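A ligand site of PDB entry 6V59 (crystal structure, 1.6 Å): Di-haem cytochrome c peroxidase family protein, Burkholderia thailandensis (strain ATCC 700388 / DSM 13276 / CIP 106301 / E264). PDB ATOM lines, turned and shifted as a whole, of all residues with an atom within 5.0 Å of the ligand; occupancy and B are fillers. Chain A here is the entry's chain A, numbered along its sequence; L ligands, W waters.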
ATOM      1  N   PHE A 109       8.957  14.388  29.923  1.00  0.00           N
ATOM      2  CA  PHE A 109       9.363  14.261  28.526  1.00  0.00           C
ATOM      3  C   PHE A 109       9.594  15.614  27.872  1.00  0.00           C
ATOM      4  O   PHE A 109      10.453  15.746  27.001  1.00  0.00           O
ATOM      5  CB  PHE A 109       8.300  13.468  27.766  1.00  0.00           C
ATOM      6  CG  PHE A 109       8.736  13.018  26.391  1.00  0.00           C
ATOM      7  CD1 PHE A 109       8.489  13.795  25.279  1.00  0.00           C
ATOM      8  CD2 PHE A 109       9.370  11.798  26.227  1.00  0.00           C
ATOM      9  CE1 PHE A 109       8.885  13.364  24.023  1.00  0.00           C
ATOM     10  CE2 PHE A 109       9.777  11.373  24.977  1.00  0.00           C
ATOM     11  CZ  PHE A 109       9.530  12.150  23.866  1.00  0.00           C
ATOM     12  N   MET A 120      17.098  21.638  26.410  1.00  0.00           N
ATOM     13  CA  MET A 120      16.846  20.439  25.620  1.00  0.00           C
ATOM     14  C   MET A 120      16.007  19.471  26.449  1.00  0.00           C
ATOM     15  O   MET A 120      16.384  19.129  27.570  1.00  0.00           O
ATOM     16  CB  MET A 120      18.156  19.785  25.177  1.00  0.00           C
ATOM     17  CG  MET A 120      18.062  18.324  24.782  1.00  0.00           C
ATOM     18  SD  MET A 120      19.523  17.743  23.894  1.00  0.00           S
ATOM     19  CE  MET A 120      19.075  18.227  22.245  1.00  0.00           C
ATOM     20  N   SER A 121      14.872  19.060  25.907  1.00  0.00           N
ATOM     21  CA  SER A 121      14.033  18.037  26.497  1.00  0.00           C
ATOM     22  C   SER A 121      14.102  16.778  25.651  1.00  0.00           C
ATOM     23  O   SER A 121      14.711  16.756  24.586  1.00  0.00           O
ATOM     24  CB  SER A 121      12.585  18.525  26.610  1.00  0.00           C
ATOM     25  OG  SER A 121      11.993  18.569  25.321  1.00  0.00           O
ATOM     26  N   CYS A 122      13.453  15.713  26.148  1.00  0.00           N
ATOM     27  CA  CYS A 122      13.303  14.512  25.308  1.00  0.00           C
ATOM     28  C   CYS A 122      12.725  14.881  23.947  1.00  0.00           C
ATOM     29  O   CYS A 122      13.125  14.320  22.922  1.00  0.00           O
ATOM     30  CB  CYS A 122      12.381  13.488  25.983  1.00  0.00           C
ATOM     31  SG  CYS A 122      12.764  13.057  27.687  1.00  0.00           S
ATOM     32  N   SER A 124      13.150  17.333  22.148  1.00  0.00           N
ATOM     33  CA  SER A 124      14.124  17.919  21.239  1.00  0.00           C
ATOM     34  C   SER A 124      14.676  16.922  20.234  1.00  0.00           C
ATOM     35  O   SER A 124      15.244  17.342  19.212  1.00  0.00           O
ATOM     36  CB  SER A 124      15.286  18.513  22.039  1.00  0.00           C
ATOM     37  OG  SER A 124      14.818  19.506  22.946  1.00  0.00           O
ATOM     38  N   CYS A 125      14.566  15.638  20.519  1.00  0.00           N
ATOM     39  CA  CYS A 125      14.967  14.586  19.598  1.00  0.00           C
ATOM     40  C   CYS A 125      13.825  13.661  19.223  1.00  0.00           C
ATOM     41  O   CYS A 125      14.035  12.730  18.440  1.00  0.00           O
ATOM     42  CB  CYS A 125      16.113  13.767  20.207  1.00  0.00           C
ATOM     43  SG  CYS A 125      17.554  14.835  20.546  1.00  0.00           S
ATOM     44  N   HIS A 126      12.623  13.900  19.773  1.00  0.00           N
ATOM     45  CA  HIS A 126      11.447  13.046  19.611  1.00  0.00           C
ATOM     46  C   HIS A 126      10.251  13.996  19.512  1.00  0.00           C
ATOM     47  O   HIS A 126       9.529  14.223  20.487  1.00  0.00           O
ATOM     48  CB  HIS A 126      11.300  12.069  20.763  1.00  0.00           C
ATOM     49  CG  HIS A 126      12.450  11.131  20.914  1.00  0.00           C
ATOM     50  ND1 HIS A 126      12.685  10.100  20.037  1.00  0.00           N
ATOM     51  CD2 HIS A 126      13.392  11.019  21.884  1.00  0.00           C
ATOM     52  CE1 HIS A 126      13.732   9.410  20.435  1.00  0.00           C
ATOM     53  NE2 HIS A 126      14.180   9.936  21.549  1.00  0.00           N
ATOM     54  N   PRO A 147      20.322  13.457  15.527  1.00  0.00           N
ATOM     55  CA  PRO A 147      19.958  14.607  16.364  1.00  0.00           C
ATOM     56  C   PRO A 147      21.174  15.317  16.945  1.00  0.00           C
ATOM     57  O   PRO A 147      22.161  14.696  17.339  1.00  0.00           O
ATOM     58  CB  PRO A 147      19.102  13.989  17.470  1.00  0.00           C
ATOM     59  CG  PRO A 147      18.561  12.738  16.893  1.00  0.00           C
ATOM     60  CD  PRO A 147      19.613  12.228  15.940  1.00  0.00           C
ATOM     61  N   GLN A 148      21.061  16.638  17.007  1.00  0.00           N
ATOM     62  CA  GLN A 148      22.014  17.432  17.762  1.00  0.00           C
ATOM     63  C   GLN A 148      21.704  17.317  19.255  1.00  0.00           C
ATOM     64  O   GLN A 148      20.548  17.334  19.664  1.00  0.00           O
ATOM     65  CB  GLN A 148      21.932  18.882  17.328  1.00  0.00           C
ATOM     66  CG  GLN A 148      22.991  19.771  17.948  1.00  0.00           C
ATOM     67  CD  GLN A 148      22.937  21.179  17.410  1.00  0.00           C
ATOM     68  OE1 GLN A 148      22.527  21.400  16.274  1.00  0.00           O
ATOM     69  NE2 GLN A 148      23.373  22.136  18.220  1.00  0.00           N
ATOM     70  N   GLY A 149      22.770  17.212  20.058  1.00  0.00           N
ATOM     71  CA  GLY A 149      22.662  17.229  21.502  1.00  0.00           C
ATOM     72  C   GLY A 149      22.570  18.629  22.072  1.00  0.00           C
ATOM     73  O   GLY A 149      22.223  19.602  21.399  1.00  0.00           O
ATOM     74  N   SER A 156      24.059  12.966  18.722  1.00  0.00           N
ATOM     75  CA  SER A 156      23.839  11.575  19.062  1.00  0.00           C
ATOM     76  C   SER A 156      24.781  10.682  18.256  1.00  0.00           C
ATOM     77  O   SER A 156      25.235  11.047  17.167  1.00  0.00           O
ATOM     78  CB  SER A 156      22.381  11.177  18.772  1.00  0.00           C
ATOM     79  OG  SER A 156      21.477  11.786  19.692  1.00  0.00           O
ATOM     80  N   ARG A 158      23.810   7.758  17.114  1.00  0.00           N
ATOM     81  CA  ARG A 158      22.930   7.083  16.186  1.00  0.00           C
ATOM     82  C   ARG A 158      21.754   7.998  15.873  1.00  0.00           C
ATOM     83  O   ARG A 158      21.533   9.022  16.531  1.00  0.00           O
ATOM     84  CB  ARG A 158      22.415   5.753  16.753  1.00  0.00           C
ATOM     85  CG  ARG A 158      23.483   4.694  16.977  1.00  0.00           C
ATOM     86  CD  ARG A 158      22.890   3.352  17.379  1.00  0.00           C
ATOM     87  NE  ARG A 158      23.943   2.349  17.547  1.00  0.00           N
ATOM     88  CZ  ARG A 158      24.105   1.585  18.628  1.00  0.00           C
ATOM     89  NH1 ARG A 158      23.286   1.662  19.671  1.00  0.00           N
ATOM     90  NH2 ARG A 158      25.106   0.717  18.665  1.00  0.00           N
ATOM     91  N   ASN A 159      20.996   7.644  14.831  1.00  0.00           N
ATOM     92  CA  ASN A 159      19.725   8.297  14.563  1.00  0.00           C
ATOM     93  C   ASN A 159      18.705   7.888  15.633  1.00  0.00           C
ATOM     94  O   ASN A 159      18.786   6.811  16.220  1.00  0.00           O
ATOM     95  CB  ASN A 159      19.225   7.918  13.167  1.00  0.00           C
ATOM     96  CG  ASN A 159      18.124   8.840  12.659  1.00  0.00           C
ATOM     97  OD1 ASN A 159      17.954   9.961  13.144  1.00  0.00           O
ATOM     98  ND2 ASN A 159      17.385   8.374  11.666  1.00  0.00           N
ATOM     99  N   ALA A 160      17.763   8.783  15.914  1.00  0.00           N
ATOM    100  CA  ALA A 160      16.716   8.505  16.896  1.00  0.00           C
ATOM    101  C   ALA A 160      15.466   8.008  16.193  1.00  0.00           C
ATOM    102  O   ALA A 160      15.083   8.575  15.154  1.00  0.00           O
ATOM    103  CB  ALA A 160      16.378   9.745  17.714  1.00  0.00           C
ATOM    104  N   PRO A 161      14.819   6.976  16.715  1.00  0.00           N
ATOM    105  CA  PRO A 161      13.584   6.475  16.107  1.00  0.00           C
ATOM    106  C   PRO A 161      12.361   7.209  16.634  1.00  0.00           C
ATOM    107  O   PRO A 161      12.421   7.936  17.623  1.00  0.00           O
ATOM    108  CB  PRO A 161      13.562   5.012  16.544  1.00  0.00           C
ATOM    109  CG  PRO A 161      14.150   5.058  17.903  1.00  0.00           C
ATOM    110  CD  PRO A 161      15.271   6.079  17.798  1.00  0.00           C
ATOM    111  N   LEU A 163       9.151   7.123  18.768  1.00  0.00           N
ATOM    112  CA  LEU A 163       8.776   6.425  19.988  1.00  0.00           C
ATOM    113  C   LEU A 163       7.337   5.943  19.982  1.00  0.00           C
ATOM    114  O   LEU A 163       6.931   5.230  20.904  1.00  0.00           O
ATOM    115  CB  LEU A 163       8.981   7.322  21.222  1.00  0.00           C
ATOM    116  CG  LEU A 163      10.433   7.795  21.418  1.00  0.00           C
ATOM    117  CD1 LEU A 163      10.604   8.537  22.728  1.00  0.00           C
ATOM    118  CD2 LEU A 163      11.400   6.618  21.341  1.00  0.00           C
ATOM    119  N   VAL A 166       6.683   2.137  20.811  1.00  0.00           N
ATOM    120  CA  VAL A 166       7.846   1.635  21.520  1.00  0.00           C
ATOM    121  C   VAL A 166       7.436   0.703  22.657  1.00  0.00           C
ATOM    122  O   VAL A 166       8.248  -0.107  23.103  1.00  0.00           O
ATOM    123  CB  VAL A 166       8.708   2.794  22.061  1.00  0.00           C
ATOM    124  CG1 VAL A 166       8.045   3.492  23.231  1.00  0.00           C
ATOM    125  CG2 VAL A 166      10.100   2.280  22.469  1.00  0.00           C
ATOM    126  N   VAL A 169       8.242  -3.142  22.264  1.00  0.00           N
ATOM    127  CA  VAL A 169       9.594  -3.724  22.234  1.00  0.00           C
ATOM    128  C   VAL A 169       9.756  -4.620  23.455  1.00  0.00           C
ATOM    129  O   VAL A 169       9.733  -4.116  24.590  1.00  0.00           O
ATOM    130  CB  VAL A 169      10.677  -2.646  22.216  1.00  0.00           C
ATOM    131  CG1 VAL A 169      12.065  -3.308  22.216  1.00  0.00           C
ATOM    132  CG2 VAL A 169      10.519  -1.737  21.006  1.00  0.00           C
ATOM    133  N   LEU A 189      15.808  -2.462  24.224  1.00  0.00           N
ATOM    134  CA  LEU A 189      15.701  -1.105  23.725  1.00  0.00           C
ATOM    135  C   LEU A 189      17.072  -0.593  23.296  1.00  0.00           C
ATOM    136  O   LEU A 189      18.104  -1.071  23.759  1.00  0.00           O
ATOM    137  CB  LEU A 189      15.106  -0.192  24.806  1.00  0.00           C
ATOM    138  CG  LEU A 189      13.622  -0.438  25.059  1.00  0.00           C
ATOM    139  CD1 LEU A 189      13.212   0.200  26.366  1.00  0.00           C
ATOM    140  CD2 LEU A 189      12.775   0.072  23.917  1.00  0.00           C
ATOM    141  N   PHE A 190      17.036   0.430  22.421  1.00  0.00           N
ATOM    142  CA  PHE A 190      18.177   0.878  21.609  1.00  0.00           C
ATOM    143  C   PHE A 190      18.477  -0.127  20.497  1.00  0.00           C
ATOM    144  O   PHE A 190      18.090  -1.308  20.570  1.00  0.00           O
ATOM    145  CB  PHE A 190      19.421   1.097  22.466  1.00  0.00           C
ATOM    146  CG  PHE A 190      19.286   2.195  23.488  1.00  0.00           C
ATOM    147  CD1 PHE A 190      19.004   3.499  23.100  1.00  0.00           C
ATOM    148  CD2 PHE A 190      19.495   1.935  24.834  1.00  0.00           C
ATOM    149  CE1 PHE A 190      18.911   4.510  24.032  1.00  0.00           C
ATOM    150  CE2 PHE A 190      19.413   2.940  25.769  1.00  0.00           C
ATOM    151  CZ  PHE A 190      19.126   4.230  25.371  1.00  0.00           C
ATOM    152  N   SER A 191      19.166   0.338  19.453  1.00  0.00           N
ATOM    153  CA  SER A 191      19.429  -0.513  18.296  1.00  0.00           C
ATOM    154  C   SER A 191      20.371  -1.664  18.621  1.00  0.00           C
ATOM    155  O   SER A 191      20.454  -2.608  17.830  1.00  0.00           O
ATOM    156  CB  SER A 191      20.023   0.309  17.156  1.00  0.00           C
ATOM    157  OG  SER A 191      19.043   1.185  16.618  1.00  0.00           O
ATOM    158  N   ASP A 192      21.070  -1.596  19.752  1.00  0.00           N
ATOM    159  CA  ASP A 192      21.941  -2.681  20.196  1.00  0.00           C
ATOM    160  C   ASP A 192      21.360  -3.416  21.394  1.00  0.00           C
ATOM    161  O   ASP A 192      22.052  -4.234  22.016  1.00  0.00           O
ATOM    162  CB  ASP A 192      23.344  -2.164  20.530  1.00  0.00           C
ATOM    163  CG  ASP A 192      23.335  -1.030  21.551  1.00  0.00           C
ATOM    164  OD1 ASP A 192      22.315  -0.827  22.235  1.00  0.00           O
ATOM    165  OD2 ASP A 192      24.389  -0.335  21.666  1.00  0.00           O
ATOM    166  N   ARG A 194      20.782  -2.645  24.436  1.00  0.00           N
ATOM    167  CA  ARG A 194      21.529  -2.574  25.679  1.00  0.00           C
ATOM    168  C   ARG A 194      20.687  -2.206  26.891  1.00  0.00           C
ATOM    169  O   ARG A 194      21.169  -2.337  28.028  1.00  0.00           O
ATOM    170  CB  ARG A 194      22.697  -1.602  25.530  1.00  0.00           C
ATOM    171  CG  ARG A 194      22.316  -0.152  25.401  1.00  0.00           C
ATOM    172  CD  ARG A 194      23.579   0.693  25.231  1.00  0.00           C
ATOM    173  NE  ARG A 194      23.315   2.127  25.229  1.00  0.00           N
ATOM    174  CZ  ARG A 194      22.900   2.810  24.162  1.00  0.00           C
ATOM    175  NH1 ARG A 194      22.704   4.123  24.249  1.00  0.00           N
ATOM    176  NH2 ARG A 194      22.693   2.196  23.003  1.00  0.00           N
ATOM    177  N   LEU A 198      12.043   0.200  29.535  1.00  0.00           N
ATOM    178  CA  LEU A 198      11.950   1.638  29.304  1.00  0.00           C
ATOM    179  C   LEU A 198      12.490   2.426  30.480  1.00  0.00           C
ATOM    180  O   LEU A 198      13.069   3.510  30.306  1.00  0.00           O
ATOM    181  CB  LEU A 198      10.495   2.019  29.014  1.00  0.00           C
ATOM    182  CG  LEU A 198       9.972   1.636  27.632  1.00  0.00           C
ATOM    183  CD1 LEU A 198       8.457   1.779  27.566  1.00  0.00           C
ATOM    184  CD2 LEU A 198      10.612   2.497  26.550  1.00  0.00           C
ATOM    185  N   GLN A 201      16.167   2.464  30.001  1.00  0.00           N
ATOM    186  CA  GLN A 201      16.584   3.256  28.846  1.00  0.00           C
ATOM    187  C   GLN A 201      16.872   4.702  29.230  1.00  0.00           C
ATOM    188  O   GLN A 201      17.769   5.327  28.649  1.00  0.00           O
ATOM    189  CB  GLN A 201      15.486   3.179  27.777  1.00  0.00           C
ATOM    190  CG  GLN A 201      15.815   3.884  26.479  1.00  0.00           C
ATOM    191  CD  GLN A 201      15.655   5.391  26.574  1.00  0.00           C
ATOM    192  OE1 GLN A 201      14.867   5.886  27.369  1.00  0.00           O
ATOM    193  NE2 GLN A 201      16.422   6.123  25.766  1.00  0.00           N
ATOM    194  N   LEU A 202      16.137   5.220  30.205  1.00  0.00           N
ATOM    195  CA  LEU A 202      16.164   6.653  30.521  1.00  0.00           C
ATOM    196  C   LEU A 202      17.559   7.119  30.914  1.00  0.00           C
ATOM    197  O   LEU A 202      17.900   8.295  30.692  1.00  0.00           O
ATOM    198  CB  LEU A 202      15.178   6.908  31.656  1.00  0.00           C
ATOM    199  CG  LEU A 202      14.809   8.351  31.986  1.00  0.00           C
ATOM    200  CD1 LEU A 202      13.769   8.860  30.995  1.00  0.00           C
ATOM    201  CD2 LEU A 202      14.283   8.405  33.401  1.00  0.00           C
ATOM    202  N   PRO A 205      20.096   8.864  27.548  1.00  0.00           N
ATOM    203  CA  PRO A 205      20.153  10.284  27.133  1.00  0.00           C
ATOM    204  C   PRO A 205      20.421  11.255  28.266  1.00  0.00           C
ATOM    205  O   PRO A 205      21.066  12.285  28.037  1.00  0.00           O
ATOM    206  CB  PRO A 205      18.764  10.513  26.498  1.00  0.00           C
ATOM    207  CG  PRO A 205      17.887   9.430  27.093  1.00  0.00           C
ATOM    208  CD  PRO A 205      18.798   8.239  27.270  1.00  0.00           C
ATOM    209  N   LEU A 206      19.970  10.945  29.486  1.00  0.00           N
ATOM    210  CA  LEU A 206      20.120  11.899  30.582  1.00  0.00           C
ATOM    211  C   LEU A 206      21.576  12.170  30.909  1.00  0.00           C
ATOM    212  O   LEU A 206      21.938  13.301  31.277  1.00  0.00           O
ATOM    213  CB  LEU A 206      19.425  11.384  31.846  1.00  0.00           C
ATOM    214  CG  LEU A 206      17.915  11.545  31.919  1.00  0.00           C
ATOM    215  CD1 LEU A 206      17.381  10.790  33.123  1.00  0.00           C
ATOM    216  CD2 LEU A 206      17.522  13.015  31.974  1.00  0.00           C
ATOM    217  N   ASP A 210      27.010  13.759  24.931  1.00  0.00           N
ATOM    218  CA  ASP A 210      26.652  14.231  23.589  1.00  0.00           C
ATOM    219  C   ASP A 210      25.151  14.416  23.413  1.00  0.00           C
ATOM    220  O   ASP A 210      24.739  14.892  22.348  1.00  0.00           O
ATOM    221  CB  ASP A 210      27.185  13.254  22.528  1.00  0.00           C
ATOM    222  CG  ASP A 210      28.698  13.341  22.360  1.00  0.00           C
ATOM    223  OD1 ASP A 210      29.262  14.418  22.626  1.00  0.00           O
ATOM    224  OD2 ASP A 210      29.311  12.332  21.983  1.00  0.00           O
ATOM    225  N   GLU A 211      24.338  14.050  24.411  1.00  0.00           N
ATOM    226  CA  GLU A 211      22.890  14.237  24.356  1.00  0.00           C
ATOM    227  C   GLU A 211      22.486  15.237  25.459  1.00  0.00           C
ATOM    228  O   GLU A 211      22.751  16.429  25.307  1.00  0.00           O
ATOM    229  CB  GLU A 211      22.171  12.889  24.471  1.00  0.00           C
ATOM    230  CG  GLU A 211      22.653  11.927  23.383  1.00  0.00           C
ATOM    231  CD  GLU A 211      21.765  10.718  23.168  1.00  0.00           C
ATOM    232  OE1 GLU A 211      21.736  10.234  22.020  1.00  0.00           O
ATOM    233  OE2 GLU A 211      21.105  10.265  24.125  1.00  0.00           O
ATOM    234  N   MET A 212      21.873  14.784  26.552  1.00  0.00           N
ATOM    235  CA  MET A 212      21.388  15.743  27.548  1.00  0.00           C
ATOM    236  C   MET A 212      22.459  16.163  28.549  1.00  0.00           C
ATOM    237  O   MET A 212      22.334  17.237  29.144  1.00  0.00           O
ATOM    238  CB  MET A 212      20.173  15.158  28.286  1.00  0.00           C
ATOM    239  CG  MET A 212      19.050  14.810  27.311  1.00  0.00           C
ATOM    240  SD  MET A 212      17.535  14.200  28.050  1.00  0.00           S
ATOM    241  CE  MET A 212      16.694  15.746  28.426  1.00  0.00           C
ATOM    242  N   MET A 256       8.168   7.808  33.130  1.00  0.00           N
ATOM    243  CA  MET A 256       8.358   7.782  31.684  1.00  0.00           C
ATOM    244  C   MET A 256       7.791   6.504  31.085  1.00  0.00           C
ATOM    245  O   MET A 256       7.158   6.525  30.017  1.00  0.00           O
ATOM    246  CB  MET A 256       9.838   7.902  31.352  1.00  0.00           C
ATOM    247  CG  MET A 256      10.114   8.085  29.874  1.00  0.00           C
ATOM    248  SD  MET A 256       9.263   9.541  29.209  1.00  0.00           S
ATOM    249  CE  MET A 256      10.031  10.843  30.157  1.00  0.00           C
ATOM    250  N   LEU A 260       5.060   6.291  28.044  1.00  0.00           N
ATOM    251  CA  LEU A 260       5.340   5.633  26.778  1.00  0.00           C
ATOM    252  C   LEU A 260       4.522   4.359  26.597  1.00  0.00           C
ATOM    253  O   LEU A 260       4.399   3.883  25.459  1.00  0.00           O
ATOM    254  CB  LEU A 260       6.843   5.335  26.662  1.00  0.00           C
ATOM    255  CG  LEU A 260       7.723   6.599  26.606  1.00  0.00           C
ATOM    256  CD1 LEU A 260       9.204   6.239  26.521  1.00  0.00           C
ATOM    257  CD2 LEU A 260       7.345   7.523  25.458  1.00  0.00           C
ATOM    258  N   ARG A 368      18.932  -3.939  15.705  1.00  0.00           N
ATOM    259  CA  ARG A 368      17.533  -4.323  15.848  1.00  0.00           C
ATOM    260  C   ARG A 368      16.724  -3.805  14.661  1.00  0.00           C
ATOM    261  O   ARG A 368      16.793  -2.628  14.310  1.00  0.00           O
ATOM    262  CB  ARG A 368      16.937  -3.804  17.161  1.00  0.00           C
ATOM    263  CG  ARG A 368      15.795  -4.673  17.747  1.00  0.00           C
ATOM    264  CD  ARG A 368      15.126  -4.022  18.952  1.00  0.00           C
ATOM    265  NE  ARG A 368      14.317  -2.892  18.512  1.00  0.00           N
ATOM    266  CZ  ARG A 368      14.226  -1.711  19.119  1.00  0.00           C
ATOM    267  NH1 ARG A 368      14.901  -1.464  20.234  1.00  0.00           N
ATOM    268  NH2 ARG A 368      13.480  -0.750  18.578  1.00  0.00           N
HETATM  269 FE1  LIG L   1      15.734   9.205  22.949  1.00  0.00          FE
HETATM  270  C1  LIG L   1      16.258   6.073  21.599  1.00  0.00           C
HETATM  271  C2  LIG L   1      13.385   7.850  25.072  1.00  0.00           C
HETATM  272  C3  LIG L   1      15.977  11.970  25.011  1.00  0.00           C
HETATM  273  C4  LIG L   1      18.173  10.522  20.944  1.00  0.00           C
HETATM  274  N1  LIG L   1      14.878   7.364  23.170  1.00  0.00           N
HETATM  275  C5  LIG L   1      15.261   6.204  22.531  1.00  0.00           C
HETATM  276  C6  LIG L   1      14.418   5.117  23.001  1.00  0.00           C
HETATM  277  C7  LIG L   1      13.606   5.623  23.928  1.00  0.00           C
HETATM  278  C8  LIG L   1      13.913   7.025  24.109  1.00  0.00           C
HETATM  279  C9  LIG L   1      12.511   4.867  24.719  1.00  0.00           C
HETATM  280  C10 LIG L   1      14.533   3.642  22.527  1.00  0.00           C
HETATM  281  C11 LIG L   1      13.706   3.469  21.264  1.00  0.00           C
HETATM  282  C12 LIG L   1      13.898   2.118  20.639  1.00  0.00           C
HETATM  283  O1  LIG L   1      12.991   1.712  19.880  1.00  0.00           O
HETATM  284  O2  LIG L   1      14.915   1.403  20.936  1.00  0.00           O
HETATM  285  N2  LIG L   1      14.824   9.825  24.680  1.00  0.00           N
HETATM  286  C13 LIG L   1      13.862   9.109  25.384  1.00  0.00           C
HETATM  287  C14 LIG L   1      13.578   9.838  26.589  1.00  0.00           C
HETATM  288  C15 LIG L   1      14.220  11.004  26.526  1.00  0.00           C
HETATM  289  C16 LIG L   1      15.120  10.957  25.403  1.00  0.00           C
HETATM  290  C17 LIG L   1      12.451   9.435  27.560  1.00  0.00           C
HETATM  291  C18 LIG L   1      14.271  12.135  27.592  1.00  0.00           C
HETATM  292  C19 LIG L   1      14.670  11.597  28.975  1.00  0.00           C
HETATM  293  N3  LIG L   1      16.852  10.915  22.980  1.00  0.00           N
HETATM  294  C20 LIG L   1      16.665  11.981  23.832  1.00  0.00           C
HETATM  295  C21 LIG L   1      17.450  13.080  23.351  1.00  0.00           C
HETATM  296  C22 LIG L   1      18.071  12.696  22.223  1.00  0.00           C
HETATM  297  C23 LIG L   1      17.732  11.313  21.992  1.00  0.00           C
HETATM  298  C24 LIG L   1      17.400  14.491  23.967  1.00  0.00           C
HETATM  299  C25 LIG L   1      18.678  13.609  21.153  1.00  0.00           C
HETATM  300  C26 LIG L   1      19.943  14.312  21.703  1.00  0.00           C
HETATM  301  N4  LIG L   1      17.003   8.426  21.515  1.00  0.00           N
HETATM  302  C27 LIG L   1      17.967   9.175  20.837  1.00  0.00           C
HETATM  303  C28 LIG L   1      18.640   8.305  19.900  1.00  0.00           C
HETATM  304  C29 LIG L   1      18.049   6.917  20.099  1.00  0.00           C
HETATM  305  C30 LIG L   1      17.074   7.084  21.150  1.00  0.00           C
HETATM  306  C31 LIG L   1      19.859   8.641  19.043  1.00  0.00           C
HETATM  307  C32 LIG L   1      18.584   5.593  19.530  1.00  0.00           C
HETATM  308  C33 LIG L   1      19.906   5.294  20.233  1.00  0.00           C
HETATM  309  C34 LIG L   1      20.349   3.891  19.956  1.00  0.00           C
HETATM  310  O3  LIG L   1      19.576   3.135  19.318  1.00  0.00           O
HETATM  311  O4  LIG L   1      21.445   3.515  20.436  1.00  0.00           O
HETATM  312  O   HOH W   1      23.273   5.317  21.127  1.00  0.00           O
HETATM  313  O   HOH W   2      16.538   2.613  18.566  1.00  0.00           O
HETATM  314  O   HOH W   3      10.950   2.789  18.684  1.00  0.00           O
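The side-chain amide nitrogen of Gln 201 lies close to a nitrogen (N1) of the ligand (3.3 Å).
Merely in contact with the ligand: Ala 160, Pro 205, Leu 202, Asn 159, Leu 163, Leu 198, Met 256, Ser 121, Ser 156, Gln 148, Pro 161, Pro 147, Glu 211, Met 212, Leu 189, Met 120, Val 166 and Gly 149.
Hydrophobic or aromatic side chains within 4 Å of the ligand: Met 120, His 126, Pro 147, Ala 160, Pro 161, Leu 163, Val 166, Leu 189, Phe 190, Leu 198, Leu 202, Pro 205, Met 212 and Met 256.
The nearest printed residue that does not touch the ligand is Leu 260 (4.01 Å).
The backbone NH (N) of Cys 122 lies within hydrogen-bond range of the backbone carbonyl oxygen (O) of Phe 109, at 3.1 Å.
A ring nitrogen (ND1) of His 126 lies within hydrogen-bond range of the backbone carbonyl oxygen of Pro 161, 3.3 Å away.
NH1 of Arg 158 lies within salt-bridge range of OD2 of Asp 192 (3.0 Å).
The guanidinium group of Arg 368 is in hydrogen-bond range of the backbone carbonyl oxygen of Phe 190 (3.2 Å).
The backbone NH (N) of Arg 194 lies within hydrogen-bond range of the backbone carbonyl oxygen (O) of Leu 189 (3.2 Å).
The guanidinium group (NH2) of Arg 194 is in salt-bridge range of the side-chain carboxylate (OD1) of Asp 192, at 3.1 Å.
N of Ser 121 sits at hydrogen-bond distance from OG of Ser 124 (3.0 Å).
N of Ser 156 sits at hydrogen-bond distance from O of Pro 147, 2.9 Å away.
C18 of the ligand is covalently linked to SG of Cys 122, 1.8 Å away.
A carbon (C25) of the ligand is bonded to the side-chain sulfur (SG) of Cys 125 (1.8 Å).
A ring nitrogen (NE2) of His 126 binds an iron atom (FE1) of the ligand (2.2 Å).
An oxygen (O4) of the ligand lies within salt-bridge range of the guanidinium group (NH1) of Arg 158 (2.7 Å).
The backbone NH of Phe 190 sits at hydrogen-bond distance from an oxygen (O2) of the ligand (2.8 Å).
The guanidinium group (NH2) of Arg 368 lies within salt-bridge range of an oxygen (O1) of the ligand, at 2.8 Å.
The backbone NH (N) of Ser 191 lies within hydrogen-bond range of an oxygen (O3) of the ligand.
The side-chain hydroxyl of Ser 191 is in hydrogen-bond range of an oxygen (O3) of the ligand, 3.4 Å away.
NH2 of Arg 194 lies within salt-bridge range of O4 of the ligand (3.1 Å).
Water W1 bridges an oxygen (O4) of the ligand (2.7 Å) and the guanidinium group of Arg 194 (3.4 Å).
Water W2 lies within hydrogen-bond range of O2 of the ligand and OG of Ser 191.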
